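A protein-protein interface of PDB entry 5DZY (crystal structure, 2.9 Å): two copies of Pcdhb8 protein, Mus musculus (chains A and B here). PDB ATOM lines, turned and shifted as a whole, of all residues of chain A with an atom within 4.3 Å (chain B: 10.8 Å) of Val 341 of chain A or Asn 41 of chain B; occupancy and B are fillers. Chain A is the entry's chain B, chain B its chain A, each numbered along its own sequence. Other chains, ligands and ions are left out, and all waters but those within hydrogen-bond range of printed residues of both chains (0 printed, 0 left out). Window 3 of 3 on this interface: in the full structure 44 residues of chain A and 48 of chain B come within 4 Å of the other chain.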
ATOM      1  N   LYS A 317      13.678   8.049  17.345  1.00  0.00           N
ATOM      2  CA  LYS A 317      13.845   6.608  17.496  1.00  0.00           C
ATOM      3  C   LYS A 317      14.154   6.250  18.945  1.00  0.00           C
ATOM      4  O   LYS A 317      15.227   6.568  19.458  1.00  0.00           O
ATOM      5  CB  LYS A 317      14.955   6.094  16.577  1.00  0.00           C
ATOM      6  N   LEU A 318      13.204   5.587  19.598  1.00  0.00           N
ATOM      7  CA  LEU A 318      13.349   5.205  20.998  1.00  0.00           C
ATOM      8  C   LEU A 318      13.687   3.725  21.147  1.00  0.00           C
ATOM      9  O   LEU A 318      12.927   2.860  20.712  1.00  0.00           O
ATOM     10  CB  LEU A 318      12.067   5.527  21.770  1.00  0.00           C
ATOM     11  CG  LEU A 318      11.982   5.003  23.204  1.00  0.00           C
ATOM     12  CD1 LEU A 318      13.068   5.621  24.068  1.00  0.00           C
ATOM     13  CD2 LEU A 318      10.606   5.270  23.795  1.00  0.00           C
ATOM     14  N   THR A 319      14.829   3.439  21.763  1.00  0.00           N
ATOM     15  CA  THR A 319      15.232   2.058  22.008  1.00  0.00           C
ATOM     16  C   THR A 319      15.516   1.830  23.489  1.00  0.00           C
ATOM     17  O   THR A 319      16.432   2.429  24.053  1.00  0.00           O
ATOM     18  CB  THR A 319      16.475   1.673  21.187  1.00  0.00           C
ATOM     19  OG1 THR A 319      17.534   2.601  21.454  1.00  0.00           O
ATOM     20  CG2 THR A 319      16.155   1.687  19.699  1.00  0.00           C
ATOM     21  N   SER A 340      17.733   4.837  24.988  1.00  0.00           N
ATOM     22  CA  SER A 340      18.370   5.844  24.148  1.00  0.00           C
ATOM     23  C   SER A 340      17.396   6.385  23.106  1.00  0.00           C
ATOM     24  O   SER A 340      16.514   5.665  22.628  1.00  0.00           O
ATOM     25  CB  SER A 340      19.606   5.269  23.456  1.00  0.00           C
ATOM     26  OG  SER A 340      19.245   4.295  22.493  1.00  0.00           O
ATOM     27  N   VAL A 341      17.567   7.656  22.759  1.00  0.00           N
ATOM     28  CA  VAL A 341      16.737   8.301  21.750  1.00  0.00           C
ATOM     29  C   VAL A 341      17.597   8.837  20.608  1.00  0.00           C
ATOM     30  O   VAL A 341      18.745   9.231  20.814  1.00  0.00           O
ATOM     31  CB  VAL A 341      15.908   9.449  22.352  1.00  0.00           C
ATOM     32  CG1 VAL A 341      14.827   8.896  23.263  1.00  0.00           C
ATOM     33  CG2 VAL A 341      16.805  10.417  23.109  1.00  0.00           C
ATOM     34  N   SER A 342      17.039   8.842  19.401  1.00  0.00           N
ATOM     35  CA  SER A 342      17.773   9.307  18.230  1.00  0.00           C
ATOM     36  C   SER A 342      16.917  10.209  17.347  1.00  0.00           C
ATOM     37  O   SER A 342      15.690  10.123  17.364  1.00  0.00           O
ATOM     38  CB  SER A 342      18.288   8.117  17.416  1.00  0.00           C
ATOM     39  OG  SER A 342      19.034   8.552  16.295  1.00  0.00           O
ATOM     40  N   MET A 352      15.171  16.995  20.939  1.00  0.00           N
ATOM     41  CA  MET A 352      14.069  16.205  21.473  1.00  0.00           C
ATOM     42  C   MET A 352      14.055  16.161  22.998  1.00  0.00           C
ATOM     43  O   MET A 352      15.103  16.169  23.644  1.00  0.00           O
ATOM     44  CB  MET A 352      14.135  14.782  20.915  1.00  0.00           C
ATOM     45  CG  MET A 352      15.522  14.170  20.986  1.00  0.00           C
ATOM     46  SD  MET A 352      15.672  12.625  20.072  1.00  0.00           S
ATOM     47  CE  MET A 352      17.449  12.410  20.091  1.00  0.00           C
ATOM     48  N   ASN A 370      21.444  12.542  24.774  1.00  0.00           N
ATOM     49  CA  ASN A 370      20.378  11.747  24.169  1.00  0.00           C
ATOM     50  C   ASN A 370      20.399  10.311  24.684  1.00  0.00           C
ATOM     51  O   ASN A 370      20.146   9.365  23.939  1.00  0.00           O
ATOM     52  CB  ASN A 370      20.488  11.765  22.642  1.00  0.00           C
ATOM     53  CG  ASN A 370      20.335  13.158  22.065  1.00  0.00           C
ATOM     54  OD1 ASN A 370      19.654  14.008  22.638  1.00  0.00           O
ATOM     55  ND2 ASN A 370      20.971  13.398  20.924  1.00  0.00           N
ATOM     56  N   TYR A 372      19.223   8.570  28.390  1.00  0.00           N
ATOM     57  CA  TYR A 372      18.675   8.750  29.729  1.00  0.00           C
ATOM     58  C   TYR A 372      18.562   7.430  30.486  1.00  0.00           C
ATOM     59  O   TYR A 372      18.736   6.356  29.911  1.00  0.00           O
ATOM     60  CB  TYR A 372      17.301   9.420  29.652  1.00  0.00           C
ATOM     61  CG  TYR A 372      17.283  10.714  28.868  1.00  0.00           C
ATOM     62  CD1 TYR A 372      17.112  10.712  27.489  1.00  0.00           C
ATOM     63  CD2 TYR A 372      17.427  11.937  29.508  1.00  0.00           C
ATOM     64  CE1 TYR A 372      17.094  11.892  26.769  1.00  0.00           C
ATOM     65  CE2 TYR A 372      17.410  13.122  28.798  1.00  0.00           C
ATOM     66  CZ  TYR A 372      17.243  13.094  27.429  1.00  0.00           C
ATOM     67  OH  TYR A 372      17.224  14.272  26.718  1.00  0.00           O
ATOM     68  N   VAL A 394       8.743  10.576  24.084  1.00  0.00           N
ATOM     69  CA  VAL A 394       9.756  11.449  23.504  1.00  0.00           C
ATOM     70  C   VAL A 394       9.206  12.208  22.299  1.00  0.00           C
ATOM     71  O   VAL A 394       8.572  11.623  21.421  1.00  0.00           O
ATOM     72  CB  VAL A 394      11.002  10.652  23.080  1.00  0.00           C
ATOM     73  CG1 VAL A 394      12.141  11.595  22.730  1.00  0.00           C
ATOM     74  CG2 VAL A 394      11.419   9.705  24.191  1.00  0.00           C
ATOM     75  N   ILE B  38      25.358  -4.873  24.493  1.00  0.00           N
ATOM     76  CA  ILE B  38      25.671  -3.742  23.630  1.00  0.00           C
ATOM     77  C   ILE B  38      24.387  -3.103  23.103  1.00  0.00           C
ATOM     78  O   ILE B  38      23.473  -3.791  22.647  1.00  0.00           O
ATOM     79  CB  ILE B  38      26.589  -4.160  22.455  1.00  0.00           C
ATOM     80  CG1 ILE B  38      26.864  -2.968  21.536  1.00  0.00           C
ATOM     81  CG2 ILE B  38      25.992  -5.328  21.679  1.00  0.00           C
ATOM     82  CD1 ILE B  38      27.834  -3.274  20.416  1.00  0.00           C
ATOM     83  N   HIS B  39      24.323  -1.780  23.187  1.00  0.00           N
ATOM     84  CA  HIS B  39      23.128  -1.039  22.808  1.00  0.00           C
ATOM     85  C   HIS B  39      23.454   0.054  21.795  1.00  0.00           C
ATOM     86  O   HIS B  39      24.414   0.815  21.965  1.00  0.00           O
ATOM     87  CB  HIS B  39      22.464  -0.437  24.048  1.00  0.00           C
ATOM     88  CG  HIS B  39      21.091   0.106  23.797  1.00  0.00           C
ATOM     89  ND1 HIS B  39      20.709   1.373  24.182  1.00  0.00           N
ATOM     90  CD2 HIS B  39      20.009  -0.446  23.198  1.00  0.00           C
ATOM     91  CE1 HIS B  39      19.451   1.577  23.834  1.00  0.00           C
ATOM     92  NE2 HIS B  39      19.004   0.489  23.233  1.00  0.00           N
ATOM     93  N   HIS B  40      22.645   0.122  20.744  1.00  0.00           N
ATOM     94  CA  HIS B  40      22.836   1.088  19.669  1.00  0.00           C
ATOM     95  C   HIS B  40      21.548   1.261  18.870  1.00  0.00           C
ATOM     96  O   HIS B  40      20.680   0.388  18.881  1.00  0.00           O
ATOM     97  CB  HIS B  40      23.972   0.643  18.745  1.00  0.00           C
ATOM     98  CG  HIS B  40      23.722  -0.668  18.069  1.00  0.00           C
ATOM     99  ND1 HIS B  40      23.831  -1.877  18.724  1.00  0.00           N
ATOM    100  CD2 HIS B  40      23.366  -0.962  16.796  1.00  0.00           C
ATOM    101  CE1 HIS B  40      23.554  -2.857  17.884  1.00  0.00           C
ATOM    102  NE2 HIS B  40      23.268  -2.330  16.707  1.00  0.00           N
ATOM    103  N   ASN B  41      21.430   2.389  18.178  1.00  0.00           N
ATOM    104  CA  ASN B  41      20.252   2.660  17.360  1.00  0.00           C
ATOM    105  C   ASN B  41      20.510   2.395  15.882  1.00  0.00           C
ATOM    106  O   ASN B  41      19.671   2.693  15.033  1.00  0.00           O
ATOM    107  CB  ASN B  41      19.785   4.102  17.558  1.00  0.00           C
ATOM    108  CG  ASN B  41      19.334   4.380  18.978  1.00  0.00           C
ATOM    109  OD1 ASN B  41      18.916   3.472  19.697  1.00  0.00           O
ATOM    110  ND2 ASN B  41      19.414   5.639  19.389  1.00  0.00           N
ATOM    111  N   GLY B  42      21.678   1.832  15.582  1.00  0.00           N
ATOM    112  CA  GLY B  42      22.042   1.514  14.215  1.00  0.00           C
ATOM    113  C   GLY B  42      21.156   0.434  13.625  1.00  0.00           C
ATOM    114  O   GLY B  42      20.727  -0.480  14.330  1.00  0.00           O
ATOM    115  N   ASN B  43      20.882   0.544  12.329  1.00  0.00           N
ATOM    116  CA  ASN B  43      20.036  -0.421  11.634  1.00  0.00           C
ATOM    117  C   ASN B  43      20.649  -1.817  11.661  1.00  0.00           C
ATOM    118  O   ASN B  43      19.961  -2.803  11.922  1.00  0.00           O
ATOM    119  CB  ASN B  43      19.799   0.029  10.188  1.00  0.00           C
ATOM    120  CG  ASN B  43      18.686  -0.749   9.504  1.00  0.00           C
ATOM    121  OD1 ASN B  43      18.679  -1.980   9.497  1.00  0.00           O
ATOM    122  ND2 ASN B  43      17.735  -0.026   8.922  1.00  0.00           N
ATOM    123  N   LYS B  44      21.947  -1.891  11.391  1.00  0.00           N
ATOM    124  CA  LYS B  44      22.657  -3.163  11.386  1.00  0.00           C
ATOM    125  C   LYS B  44      23.609  -3.264  12.573  1.00  0.00           C
ATOM    126  O   LYS B  44      24.287  -2.297  12.918  1.00  0.00           O
ATOM    127  CB  LYS B  44      23.426  -3.339  10.075  1.00  0.00           C
ATOM    128  CG  LYS B  44      24.179  -4.655   9.963  1.00  0.00           C
ATOM    129  CD  LYS B  44      23.229  -5.841  10.008  1.00  0.00           C
ATOM    130  CE  LYS B  44      22.264  -5.818   8.833  1.00  0.00           C
ATOM    131  NZ  LYS B  44      22.979  -5.850   7.527  1.00  0.00           N
ATOM    132  N   GLU B  45      23.649  -4.435  13.199  1.00  0.00           N
ATOM    133  CA  GLU B  45      24.564  -4.672  14.308  1.00  0.00           C
ATOM    134  C   GLU B  45      25.943  -5.048  13.778  1.00  0.00           C
ATOM    135  O   GLU B  45      26.231  -6.222  13.548  1.00  0.00           O
ATOM    136  CB  GLU B  45      24.028  -5.769  15.230  1.00  0.00           C
ATOM    137  CG  GLU B  45      24.797  -5.914  16.533  1.00  0.00           C
ATOM    138  CD  GLU B  45      24.239  -7.009  17.421  1.00  0.00           C
ATOM    139  OE1 GLU B  45      24.165  -8.168  16.964  1.00  0.00           O
ATOM    140  OE2 GLU B  45      23.871  -6.708  18.576  1.00  0.00           O
ATOM    141  N   LEU B  46      26.788  -4.042  13.581  1.00  0.00           N
ATOM    142  CA  LEU B  46      28.123  -4.249  13.028  1.00  0.00           C
ATOM    143  C   LEU B  46      29.028  -5.020  13.984  1.00  0.00           C
ATOM    144  O   LEU B  46      29.907  -5.765  13.551  1.00  0.00           O
ATOM    145  CB  LEU B  46      28.774  -2.908  12.678  1.00  0.00           C
ATOM    146  CG  LEU B  46      28.465  -2.261  11.324  1.00  0.00           C
ATOM    147  CD1 LEU B  46      27.017  -1.807  11.229  1.00  0.00           C
ATOM    148  CD2 LEU B  46      29.411  -1.096  11.070  1.00  0.00           C
ATOM    149  N   LEU B  47      28.809  -4.839  15.281  1.00  0.00           N
ATOM    150  CA  LEU B  47      29.689  -5.421  16.287  1.00  0.00           C
ATOM    151  C   LEU B  47      29.001  -6.470  17.153  1.00  0.00           C
ATOM    152  O   LEU B  47      27.902  -6.252  17.663  1.00  0.00           O
ATOM    153  CB  LEU B  47      30.265  -4.322  17.180  1.00  0.00           C
ATOM    154  CG  LEU B  47      31.250  -3.357  16.520  1.00  0.00           C
ATOM    155  CD1 LEU B  47      31.523  -2.178  17.430  1.00  0.00           C
ATOM    156  CD2 LEU B  47      32.544  -4.071  16.177  1.00  0.00           C
ATOM    157  N   LEU B  76      31.147   5.922  14.236  1.00  0.00           N
ATOM    158  CA  LEU B  76      29.898   5.359  14.737  1.00  0.00           C
ATOM    159  C   LEU B  76      29.922   5.250  16.258  1.00  0.00           C
ATOM    160  O   LEU B  76      30.807   4.612  16.829  1.00  0.00           O
ATOM    161  CB  LEU B  76      29.637   3.988  14.112  1.00  0.00           C
ATOM    162  N   HIS B  77      28.946   5.875  16.909  1.00  0.00           N
ATOM    163  CA  HIS B  77      28.879   5.875  18.366  1.00  0.00           C
ATOM    164  C   HIS B  77      27.865   4.863  18.887  1.00  0.00           C
ATOM    165  O   HIS B  77      26.703   4.862  18.479  1.00  0.00           O
ATOM    166  CB  HIS B  77      28.541   7.277  18.882  1.00  0.00           C
ATOM    167  CG  HIS B  77      27.283   7.848  18.306  1.00  0.00           C
ATOM    168  ND1 HIS B  77      26.028   7.457  18.721  1.00  0.00           N
ATOM    169  CD2 HIS B  77      27.087   8.782  17.344  1.00  0.00           C
ATOM    170  CE1 HIS B  77      25.113   8.125  18.042  1.00  0.00           C
ATOM    171  NE2 HIS B  77      25.729   8.935  17.199  1.00  0.00           N
ATOM    172  N   PHE B  78      28.316   3.997  19.789  1.00  0.00           N
ATOM    173  CA  PHE B  78      27.449   2.996  20.405  1.00  0.00           C
ATOM    174  C   PHE B  78      27.721   2.944  21.903  1.00  0.00           C
ATOM    175  O   PHE B  78      28.726   3.478  22.366  1.00  0.00           O
ATOM    176  CB  PHE B  78      27.665   1.623  19.764  1.00  0.00           C
ATOM    177  CG  PHE B  78      29.091   1.151  19.805  1.00  0.00           C
ATOM    178  CD1 PHE B  78      29.536   0.338  20.834  1.00  0.00           C
ATOM    179  CD2 PHE B  78      29.986   1.519  18.813  1.00  0.00           C
ATOM    180  CE1 PHE B  78      30.846  -0.097  20.876  1.00  0.00           C
ATOM    181  CE2 PHE B  78      31.298   1.089  18.850  1.00  0.00           C
ATOM    182  CZ  PHE B  78      31.729   0.280  19.883  1.00  0.00           C
ATOM    183  N   GLN B  79      26.838   2.307  22.667  1.00  0.00           N
ATOM    184  CA  GLN B  79      27.020   2.273  24.116  1.00  0.00           C
ATOM    185  C   GLN B  79      26.865   0.870  24.699  1.00  0.00           C
ATOM    186  O   GLN B  79      25.816   0.245  24.574  1.00  0.00           O
ATOM    187  CB  GLN B  79      26.044   3.238  24.802  1.00  0.00           C
ATOM    188  CG  GLN B  79      24.573   3.044  24.447  1.00  0.00           C
ATOM    189  CD  GLN B  79      24.175   3.735  23.157  1.00  0.00           C
ATOM    190  OE1 GLN B  79      25.003   4.356  22.490  1.00  0.00           O
ATOM    191  NE2 GLN B  79      22.900   3.634  22.800  1.00  0.00           N
ATOM    192  N   ILE B  80      27.922   0.381  25.341  1.00  0.00           N
ATOM    193  CA  ILE B  80      27.875  -0.921  25.995  1.00  0.00           C
ATOM    194  C   ILE B  80      27.516  -0.770  27.472  1.00  0.00           C
ATOM    195  O   ILE B  80      28.013   0.126  28.158  1.00  0.00           O
ATOM    196  CB  ILE B  80      29.215  -1.677  25.860  1.00  0.00           C
ATOM    197  CG1 ILE B  80      30.383  -0.793  26.301  1.00  0.00           C
ATOM    198  CG2 ILE B  80      29.420  -2.138  24.427  1.00  0.00           C
ATOM    199  CD1 ILE B  80      31.730  -1.477  26.225  1.00  0.00           C
ATOM    200  N   GLN B  90      30.329   4.567  26.726  1.00  0.00           N
ATOM    201  CA  GLN B  90      30.145   5.020  25.354  1.00  0.00           C
ATOM    202  C   GLN B  90      31.427   4.843  24.548  1.00  0.00           C
ATOM    203  O   GLN B  90      32.488   5.336  24.931  1.00  0.00           O
ATOM    204  CB  GLN B  90      29.698   6.482  25.322  1.00  0.00           C
ATOM    205  CG  GLN B  90      29.438   7.017  23.922  1.00  0.00           C
ATOM    206  CD  GLN B  90      28.913   8.439  23.927  1.00  0.00           C
ATOM    207  OE1 GLN B  90      28.726   9.040  24.985  1.00  0.00           O
ATOM    208  NE2 GLN B  90      28.674   8.985  22.741  1.00  0.00           N
ATOM    209  N   THR B  91      31.318   4.136  23.429  1.00  0.00           N
ATOM    210  CA  THR B  91      32.468   3.854  22.580  1.00  0.00           C
ATOM    211  C   THR B  91      32.220   4.311  21.143  1.00  0.00           C
ATOM    212  O   THR B  91      31.127   4.130  20.598  1.00  0.00           O
ATOM    213  CB  THR B  91      32.810   2.350  22.585  1.00  0.00           C
ATOM    214  OG1 THR B  91      32.878   1.878  23.937  1.00  0.00           O
ATOM    215  CG2 THR B  91      34.142   2.094  21.894  1.00  0.00           C
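The side-chain hydroxyl (OG1) of Thr 319 of chain A is in hydrogen-bond range of a ring nitrogen (NE2) of His 39 of chain B (3.1 Å).
The side-chain hydroxyl (OG) of Ser 340 of chain A lies within hydrogen-bond range of the side-chain amide oxygen (OD1) of Asn 41 of chain B.
The side-chain hydroxyl (OG1) of Thr 319 of chain A sits close to the side-chain amide oxygen (OD1) of Asn 41 of chain B (2.4 Å).
N of His 39 of chain B sits at hydrogen-bond distance from O of Gln 79 of chain B, at 2.9 Å.
The backbone NH (N) of Lys 317 of chain A sits at hydrogen-bond distance from the backbone carbonyl oxygen (O) of Ser 342 of chain A (2.9 Å).
The side-chain hydroxyl (OG) of Ser 340 of chain A lies within hydrogen-bond range of the side-chain hydroxyl (OG1) of Thr 319 of chain A.
The backbone carbonyl oxygen of Asn 370 of chain A is in hydrogen-bond range of the backbone NH of Val 341 of chain A.
Among the printed residues, merely in contact across the chains: Ser 340 of chain A with His 39 of chain B (3.0 Å), Ser 340 of chain A with Gln 79 of chain B (3.7 Å), Val 341 of chain A with Asn 41 of chain B (3.9 Å) and Ser 342 of chain A with Asn 41 of chain B (3.4 Å).
Lys 317 of chain A touches none of the printed residues of chain B.
No residue of chain B comes within 4 Å of Leu 318 of chain A.
Thr 319 of chain A touches two residues of chain B.
Of chain B, only Asn 41 comes within 4 Å of Val 341 of chain A.
Asn 370 of chain A touches none of the printed residues of chain B.
Printed residues of chain A within 4 Å of His 39 of chain B: Thr 319 (3.1 Å) and Ser 340 (3.0 Å).
Asn 41 of chain B touches just these residues of chain A: Thr 319 (2.4 Å), Ser 340 (2.9 Å), Val 341 (3.9 Å) and Ser 342 (3.4 Å).
Asn 43 of chain B touches none of the printed residues of chain A.
Phe 78 of chain B touches none of the printed residues of chain A.
Printed residues of chain A within 4 Å of Gln 79 of chain B: Ser 340.
The nearest printed residue of chain A that does not touch His 39 of chain B is Val 341 of chain A (6.5 Å).
Of the 17 printed residues of chain B, 3 touch a printed residue of chain A.
Hydrophobic or aromatic side chains of chain B within 4 Å of the printed part of chain A: His 39.
Along chain B the printed residues that touch a printed residue of chain A span positions 39 to 79.
Among the printed residues, no Asp or Glu carboxylate lies within 4 Å of a Lys or Arg side-chain nitrogen of the other chain.
No position is printed for both chains.
Of the 7 pairs that touch across the chains among the printed residues, none has its exchanged pair printed and touching as well.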
